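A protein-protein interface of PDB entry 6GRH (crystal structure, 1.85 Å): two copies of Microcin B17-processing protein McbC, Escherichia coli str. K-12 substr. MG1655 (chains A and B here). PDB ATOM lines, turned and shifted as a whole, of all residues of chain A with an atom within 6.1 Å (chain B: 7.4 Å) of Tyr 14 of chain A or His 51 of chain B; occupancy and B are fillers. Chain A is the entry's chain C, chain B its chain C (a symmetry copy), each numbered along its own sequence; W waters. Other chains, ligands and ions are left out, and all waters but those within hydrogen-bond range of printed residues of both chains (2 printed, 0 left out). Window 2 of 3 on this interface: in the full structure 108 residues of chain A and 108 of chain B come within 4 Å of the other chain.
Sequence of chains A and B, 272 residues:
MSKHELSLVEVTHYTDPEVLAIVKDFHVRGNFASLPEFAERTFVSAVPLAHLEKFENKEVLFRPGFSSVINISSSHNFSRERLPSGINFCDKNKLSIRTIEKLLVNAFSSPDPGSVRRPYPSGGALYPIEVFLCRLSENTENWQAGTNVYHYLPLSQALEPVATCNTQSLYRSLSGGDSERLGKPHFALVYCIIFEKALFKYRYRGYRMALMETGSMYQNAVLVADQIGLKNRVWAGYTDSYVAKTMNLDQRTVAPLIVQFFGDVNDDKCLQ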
ATOM      1  N   GLU A  10      -9.584   6.493  26.820  1.00  0.00           N
ATOM      2  CA  GLU A  10     -10.596   7.435  26.316  1.00  0.00           C
ATOM      3  C   GLU A  10     -11.705   7.634  27.352  1.00  0.00           C
ATOM      4  O   GLU A  10     -12.210   8.744  27.512  1.00  0.00           O
ATOM      5  CB  GLU A  10     -11.205   6.956  24.984  1.00  0.00           C
ATOM      6  CG  GLU A  10     -10.215   6.821  23.834  1.00  0.00           C
ATOM      7  CD  GLU A  10      -9.859   8.139  23.150  1.00  0.00           C
ATOM      8  OE1 GLU A  10     -10.344   9.217  23.579  1.00  0.00           O
ATOM      9  OE2 GLU A  10      -9.097   8.097  22.136  1.00  0.00           O
ATOM     10  N   VAL A  11     -12.059   6.551  28.033  1.00  0.00           N
ATOM     11  CA  VAL A  11     -13.065   6.565  29.075  1.00  0.00           C
ATOM     12  C   VAL A  11     -12.612   7.379  30.278  1.00  0.00           C
ATOM     13  O   VAL A  11     -13.366   8.239  30.761  1.00  0.00           O
ATOM     14  CB  VAL A  11     -13.466   5.125  29.490  1.00  0.00           C
ATOM     15  CG1 VAL A  11     -14.341   5.120  30.731  1.00  0.00           C
ATOM     16  CG2 VAL A  11     -14.162   4.468  28.320  1.00  0.00           C
ATOM     17  N   THR A  12     -11.384   7.149  30.750  1.00  0.00           N
ATOM     18  CA  THR A  12     -10.966   7.761  32.012  1.00  0.00           C
ATOM     19  C   THR A  12     -10.876   9.308  31.941  1.00  0.00           C
ATOM     20  O   THR A  12     -10.983   9.983  32.952  1.00  0.00           O
ATOM     21  CB  THR A  12      -9.664   7.147  32.552  1.00  0.00           C
ATOM     22  OG1 THR A  12      -9.554   7.404  33.958  1.00  0.00           O
ATOM     23  CG2 THR A  12      -8.450   7.705  31.831  1.00  0.00           C
ATOM     24  N   HIS A  13     -10.689   9.843  30.739  1.00  0.00           N
ATOM     25  CA  HIS A  13     -10.761  11.279  30.508  1.00  0.00           C
ATOM     26  C   HIS A  13     -12.015  11.943  31.117  1.00  0.00           C
ATOM     27  O   HIS A  13     -11.950  13.097  31.514  1.00  0.00           O
ATOM     28  CB  HIS A  13     -10.663  11.544  28.995  1.00  0.00           C
ATOM     29  CG  HIS A  13     -10.418  12.968  28.640  1.00  0.00           C
ATOM     30  ND1 HIS A  13      -9.296  13.656  29.055  1.00  0.00           N
ATOM     31  CD2 HIS A  13     -11.136  13.834  27.878  1.00  0.00           C
ATOM     32  CE1 HIS A  13      -9.350  14.894  28.587  1.00  0.00           C
ATOM     33  NE2 HIS A  13     -10.454  15.023  27.867  1.00  0.00           N
ATOM     34  N   TYR A  14     -13.130  11.217  31.208  1.00  0.00           N
ATOM     35  CA  TYR A  14     -14.377  11.762  31.759  1.00  0.00           C
ATOM     36  C   TYR A  14     -14.697  11.329  33.177  1.00  0.00           C
ATOM     37  O   TYR A  14     -15.739  11.702  33.696  1.00  0.00           O
ATOM     38  CB  TYR A  14     -15.556  11.384  30.855  1.00  0.00           C
ATOM     39  CG  TYR A  14     -15.423  11.965  29.468  1.00  0.00           C
ATOM     40  CD1 TYR A  14     -15.811  13.264  29.206  1.00  0.00           C
ATOM     41  CD2 TYR A  14     -14.886  11.220  28.431  1.00  0.00           C
ATOM     42  CE1 TYR A  14     -15.662  13.817  27.947  1.00  0.00           C
ATOM     43  CE2 TYR A  14     -14.723  11.762  27.166  1.00  0.00           C
ATOM     44  CZ  TYR A  14     -15.133  13.060  26.930  1.00  0.00           C
ATOM     45  OH  TYR A  14     -14.997  13.604  25.700  1.00  0.00           O
ATOM     46  N   THR A  15     -13.816  10.556  33.818  1.00  0.00           N
ATOM     47  CA  THR A  15     -14.112   9.986  35.125  1.00  0.00           C
ATOM     48  C   THR A  15     -14.105  11.056  36.220  1.00  0.00           C
ATOM     49  O   THR A  15     -13.213  11.903  36.278  1.00  0.00           O
ATOM     50  CB  THR A  15     -13.117   8.842  35.448  1.00  0.00           C
ATOM     51  OG1 THR A  15     -13.429   7.745  34.586  1.00  0.00           O
ATOM     52  CG2 THR A  15     -13.188   8.403  36.902  1.00  0.00           C
ATOM     53  N   ASP A  16     -15.122  11.005  37.074  1.00  0.00           N
ATOM     54  CA  ASP A  16     -15.152  11.814  38.290  1.00  0.00           C
ATOM     55  C   ASP A  16     -14.595  10.933  39.418  1.00  0.00           C
ATOM     56  O   ASP A  16     -15.204   9.911  39.756  1.00  0.00           O
ATOM     57  CB  ASP A  16     -16.587  12.276  38.593  1.00  0.00           C
ATOM     58  CG  ASP A  16     -16.672  13.154  39.843  1.00  0.00           C
ATOM     59  OD1 ASP A  16     -15.835  13.004  40.760  1.00  0.00           O
ATOM     60  OD2 ASP A  16     -17.563  14.026  39.916  1.00  0.00           O
ATOM     61  N   LEU A 199     -19.565   4.302  34.956  1.00  0.00           N
ATOM     62  CA  LEU A 199     -19.768   5.571  35.642  1.00  0.00           C
ATOM     63  C   LEU A 199     -19.543   6.824  34.791  1.00  0.00           C
ATOM     64  O   LEU A 199     -20.085   7.892  35.105  1.00  0.00           O
ATOM     65  CB  LEU A 199     -18.881   5.626  36.893  1.00  0.00           C
ATOM     66  CG  LEU A 199     -19.205   4.532  37.930  1.00  0.00           C
ATOM     67  CD1 LEU A 199     -18.144   4.506  39.015  1.00  0.00           C
ATOM     68  CD2 LEU A 199     -20.554   4.746  38.565  1.00  0.00           C
ATOM     69  N   PHE A 200     -18.735   6.713  33.734  1.00  0.00           N
ATOM     70  CA  PHE A 200     -18.213   7.918  33.097  1.00  0.00           C
ATOM     71  C   PHE A 200     -19.270   8.830  32.478  1.00  0.00           C
ATOM     72  O   PHE A 200     -19.090  10.029  32.506  1.00  0.00           O
ATOM     73  CB  PHE A 200     -17.073   7.629  32.114  1.00  0.00           C
ATOM     74  CG  PHE A 200     -17.506   7.146  30.771  1.00  0.00           C
ATOM     75  CD1 PHE A 200     -18.168   5.946  30.622  1.00  0.00           C
ATOM     76  CD2 PHE A 200     -17.198   7.877  29.644  1.00  0.00           C
ATOM     77  CE1 PHE A 200     -18.513   5.486  29.387  1.00  0.00           C
ATOM     78  CE2 PHE A 200     -17.559   7.424  28.393  1.00  0.00           C
ATOM     79  CZ  PHE A 200     -18.234   6.241  28.265  1.00  0.00           C
ATOM     80  N   LYS A 201     -20.354   8.266  31.949  1.00  0.00           N
ATOM     81  CA  LYS A 201     -21.415   9.069  31.340  1.00  0.00           C
ATOM     82  C   LYS A 201     -22.514   9.522  32.313  1.00  0.00           C
ATOM     83  O   LYS A 201     -22.908  10.721  32.337  1.00  0.00           O
ATOM     84  CB  LYS A 201     -22.071   8.292  30.181  1.00  0.00           C
ATOM     85  CG  LYS A 201     -23.149   9.109  29.445  1.00  0.00           C
ATOM     86  CD  LYS A 201     -23.734   8.417  28.227  1.00  0.00           C
ATOM     87  CE  LYS A 201     -24.799   9.285  27.558  1.00  0.00           C
ATOM     88  NZ  LYS A 201     -25.559   8.512  26.563  1.00  0.00           N
ATOM     89  N   ALA B  46     -22.230  13.225  30.961  1.00  0.00           N
ATOM     90  CA  ALA B  46     -20.984  13.908  31.239  1.00  0.00           C
ATOM     91  C   ALA B  46     -20.079  13.945  30.014  1.00  0.00           C
ATOM     92  O   ALA B  46     -19.097  14.684  29.998  1.00  0.00           O
ATOM     93  CB  ALA B  46     -20.286  13.280  32.426  1.00  0.00           C
ATOM     94  N   VAL B  47     -20.417  13.176  28.977  1.00  0.00           N
ATOM     95  CA  VAL B  47     -19.698  13.197  27.730  1.00  0.00           C
ATOM     96  C   VAL B  47     -20.453  14.084  26.696  1.00  0.00           C
ATOM     97  O   VAL B  47     -21.638  13.899  26.506  1.00  0.00           O
ATOM     98  CB  VAL B  47     -19.586  11.770  27.180  1.00  0.00           C
ATOM     99  CG1 VAL B  47     -18.777  11.754  25.894  1.00  0.00           C
ATOM    100  CG2 VAL B  47     -18.973  10.835  28.243  1.00  0.00           C
ATOM    101  N   PRO B  48     -19.762  14.993  26.009  1.00  0.00           N
ATOM    102  CA  PRO B  48     -20.474  15.793  24.993  1.00  0.00           C
ATOM    103  C   PRO B  48     -21.034  14.922  23.882  1.00  0.00           C
ATOM    104  O   PRO B  48     -20.399  13.932  23.501  1.00  0.00           O
ATOM    105  CB  PRO B  48     -19.396  16.731  24.473  1.00  0.00           C
ATOM    106  CG  PRO B  48     -18.418  16.843  25.594  1.00  0.00           C
ATOM    107  CD  PRO B  48     -18.408  15.506  26.261  1.00  0.00           C
ATOM    108  N   LEU B  49     -22.222  15.274  23.393  1.00  0.00           N
ATOM    109  CA  LEU B  49     -22.928  14.493  22.349  1.00  0.00           C
ATOM    110  C   LEU B  49     -22.048  14.103  21.163  1.00  0.00           C
ATOM    111  O   LEU B  49     -22.129  12.972  20.685  1.00  0.00           O
ATOM    112  CB  LEU B  49     -24.165  15.263  21.822  1.00  0.00           C
ATOM    113  CG  LEU B  49     -25.126  14.550  20.839  1.00  0.00           C
ATOM    114  CD1 LEU B  49     -25.971  13.502  21.563  1.00  0.00           C
ATOM    115  CD2 LEU B  49     -26.026  15.554  20.114  1.00  0.00           C
ATOM    116  N   ALA B  50     -21.206  15.033  20.722  1.00  0.00           N
ATOM    117  CA  ALA B  50     -20.327  14.849  19.554  1.00  0.00           C
ATOM    118  C   ALA B  50     -19.239  13.795  19.735  1.00  0.00           C
ATOM    119  O   ALA B  50     -18.669  13.334  18.756  1.00  0.00           O
ATOM    120  CB  ALA B  50     -19.675  16.168  19.189  1.00  0.00           C
ATOM    121  N   HIS B  51     -18.914  13.454  20.976  1.00  0.00           N
ATOM    122  CA  HIS B  51     -17.906  12.438  21.259  1.00  0.00           C
ATOM    123  C   HIS B  51     -18.482  11.097  21.701  1.00  0.00           C
ATOM    124  O   HIS B  51     -17.719  10.150  21.925  1.00  0.00           O
ATOM    125  CB  HIS B  51     -16.948  12.967  22.325  1.00  0.00           C
ATOM    126  CG  HIS B  51     -16.094  14.091  21.842  1.00  0.00           C
ATOM    127  ND1 HIS B  51     -16.198  15.371  22.336  1.00  0.00           N
ATOM    128  CD2 HIS B  51     -15.136  14.132  20.888  1.00  0.00           C
ATOM    129  CE1 HIS B  51     -15.326  16.148  21.728  1.00  0.00           C
ATOM    130  NE2 HIS B  51     -14.671  15.421  20.841  1.00  0.00           N
ATOM    131  N   LEU B  52     -19.803  10.990  21.817  1.00  0.00           N
ATOM    132  CA  LEU B  52     -20.416   9.762  22.325  1.00  0.00           C
ATOM    133  C   LEU B  52     -20.269   8.583  21.375  1.00  0.00           C
ATOM    134  O   LEU B  52     -20.185   7.448  21.834  1.00  0.00           O
ATOM    135  CB  LEU B  52     -21.897   9.972  22.663  1.00  0.00           C
ATOM    136  CG  LEU B  52     -22.205  10.597  24.011  1.00  0.00           C
ATOM    137  CD1 LEU B  52     -23.696  10.900  24.103  1.00  0.00           C
ATOM    138  CD2 LEU B  52     -21.803   9.669  25.158  1.00  0.00           C
ATOM    139  N   GLU B  53     -20.197   8.850  20.067  1.00  0.00           N
ATOM    140  CA  GLU B  53     -20.100   7.781  19.068  1.00  0.00           C
ATOM    141  C   GLU B  53     -18.925   6.835  19.337  1.00  0.00           C
ATOM    142  O   GLU B  53     -19.065   5.607  19.203  1.00  0.00           O
ATOM    143  CB  GLU B  53     -20.000   8.349  17.639  1.00  0.00           C
ATOM    144  CG  GLU B  53     -20.344   7.340  16.528  1.00  0.00           C
ATOM    145  CD  GLU B  53     -19.211   6.383  16.133  1.00  0.00           C
ATOM    146  OE1 GLU B  53     -18.034   6.645  16.475  1.00  0.00           O
ATOM    147  OE2 GLU B  53     -19.488   5.352  15.460  1.00  0.00           O
ATOM    148  N   LYS B  54     -17.784   7.396  19.737  1.00  0.00           N
ATOM    149  CA  LYS B  54     -16.595   6.589  19.990  1.00  0.00           C
ATOM    150  C   LYS B  54     -16.750   5.584  21.156  1.00  0.00           C
ATOM    151  O   LYS B  54     -15.974   4.637  21.260  1.00  0.00           O
ATOM    152  CB  LYS B  54     -15.344   7.476  20.167  1.00  0.00           C
ATOM    153  CG  LYS B  54     -14.888   7.748  21.602  1.00  0.00           C
ATOM    154  CD  LYS B  54     -13.430   8.219  21.663  1.00  0.00           C
ATOM    155  CE  LYS B  54     -13.224   9.623  21.130  1.00  0.00           C
ATOM    156  NZ  LYS B  54     -13.867  10.631  22.024  1.00  0.00           N
ATOM    157  N   PHE B  55     -17.737   5.795  22.025  1.00  0.00           N
ATOM    158  CA  PHE B  55     -17.977   4.931  23.169  1.00  0.00           C
ATOM    159  C   PHE B  55     -19.095   3.902  23.002  1.00  0.00           C
ATOM    160  O   PHE B  55     -19.175   2.948  23.773  1.00  0.00           O
ATOM    161  CB  PHE B  55     -18.264   5.784  24.388  1.00  0.00           C
ATOM    162  CG  PHE B  55     -17.149   6.709  24.728  1.00  0.00           C
ATOM    163  CD1 PHE B  55     -15.986   6.221  25.352  1.00  0.00           C
ATOM    164  CD2 PHE B  55     -17.227   8.060  24.429  1.00  0.00           C
ATOM    165  CE1 PHE B  55     -14.948   7.077  25.678  1.00  0.00           C
ATOM    166  CE2 PHE B  55     -16.186   8.922  24.776  1.00  0.00           C
ATOM    167  CZ  PHE B  55     -15.047   8.430  25.382  1.00  0.00           C
ATOM    168  N   GLU B  56     -19.942   4.098  21.998  1.00  0.00           N
ATOM    169  CA  GLU B  56     -21.142   3.314  21.827  1.00  0.00           C
ATOM    170  C   GLU B  56     -20.820   2.035  21.030  1.00  0.00           C
ATOM    171  O   GLU B  56     -20.130   2.083  20.001  1.00  0.00           O
ATOM    172  CB  GLU B  56     -22.213   4.161  21.124  1.00  0.00           C
ATOM    173  CG  GLU B  56     -22.728   5.290  22.018  1.00  0.00           C
ATOM    174  CD  GLU B  56     -23.554   6.350  21.290  1.00  0.00           C
ATOM    175  OE1 GLU B  56     -23.630   6.361  20.047  1.00  0.00           O
ATOM    176  OE2 GLU B  56     -24.104   7.212  21.971  1.00  0.00           O
HETATM  177  O   HOH W   1     -24.038   6.963  24.727  1.00  0.00           O
HETATM  178  O   HOH W   2     -13.602  12.120  24.074  1.00  0.00           O
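Lys 54 of chain B touches Glu 10 of chain A. O of Glu 10 of chain A touches CZ of Phe 55 of chain B, at 3.6 Å. Phe 55 of chain B touches Val 11 of chain A (CE1 to N, 3.8 Å). Tyr 14 of chain A touches Ala 46 of chain B (CD1 to O, 3.7 Å). CD of Pro 48 of chain B touches CE1 of Tyr 14 of chain A (3.6 Å). Tyr 14 of chain A touches His 51 of chain B. Tyr 14 of chain A touches Phe 55 of chain B. CB of Ala 46 of chain B touches O of Phe 200 of chain A, at 3.5 Å. Val 47 of chain B touches Phe 200 of chain A. Phe 200 of chain A touches Phe 55 of chain B.
O of Lys 201 of chain A is in hydrogen-bond range of N of Ala 46 of chain B (2.9 Å).
Water W2 bridges NZ of Lys 54 of chain B (2.5 Å) and OH of Tyr 14 of chain A (2.6 Å). Water W1 lies within hydrogen-bond range of OE2 of Glu 56 of chain B and NZ of Lys 201 of chain A.
Printed residues of chain B that touch a printed residue of chain A: Ala 46, Val 47, Pro 48, His 51, Leu 52, Lys 54 and Phe 55. Printed residues of chain A that touch a printed residue of chain B: Glu 10, Val 11, Tyr 14, Phe 200 and Lys 201. Among the printed residues, 13 pairs touch across the chains.
No position is printed for both chains. Of the 13 pairs that touch across the chains among the printed residues, none has its exchanged pair printed and touching as well.
Leu 199 of chain A touches none of the printed residues of chain B. Of the printed residues of chain B, Lys 201 of chain A touches Ala 46 and Leu 52. Of the printed residues of chain A, Pro 48 of chain B touches Tyr 14 (3.6 Å). Of chain A, only Tyr 14 (3.95 Å) comes within 4 Å of His 51 of chain B. Of the printed residues of chain A, Leu 52 of chain B touches Lys 201 (3.8 Å). Of the printed residues of chain A, Lys 54 of chain B touches Glu 10. Printed residues of chain A within 4 Å of Phe 55 of chain B: Glu 10, Val 11, Tyr 14 and Phe 200. The nearest residue of chain B that does not touch Tyr 14 of chain A is Lys 54 of chain B (4.9 Å). The nearest printed residue of chain A that does not touch Lys 54 of chain B is Tyr 14 of chain A (4.9 Å).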
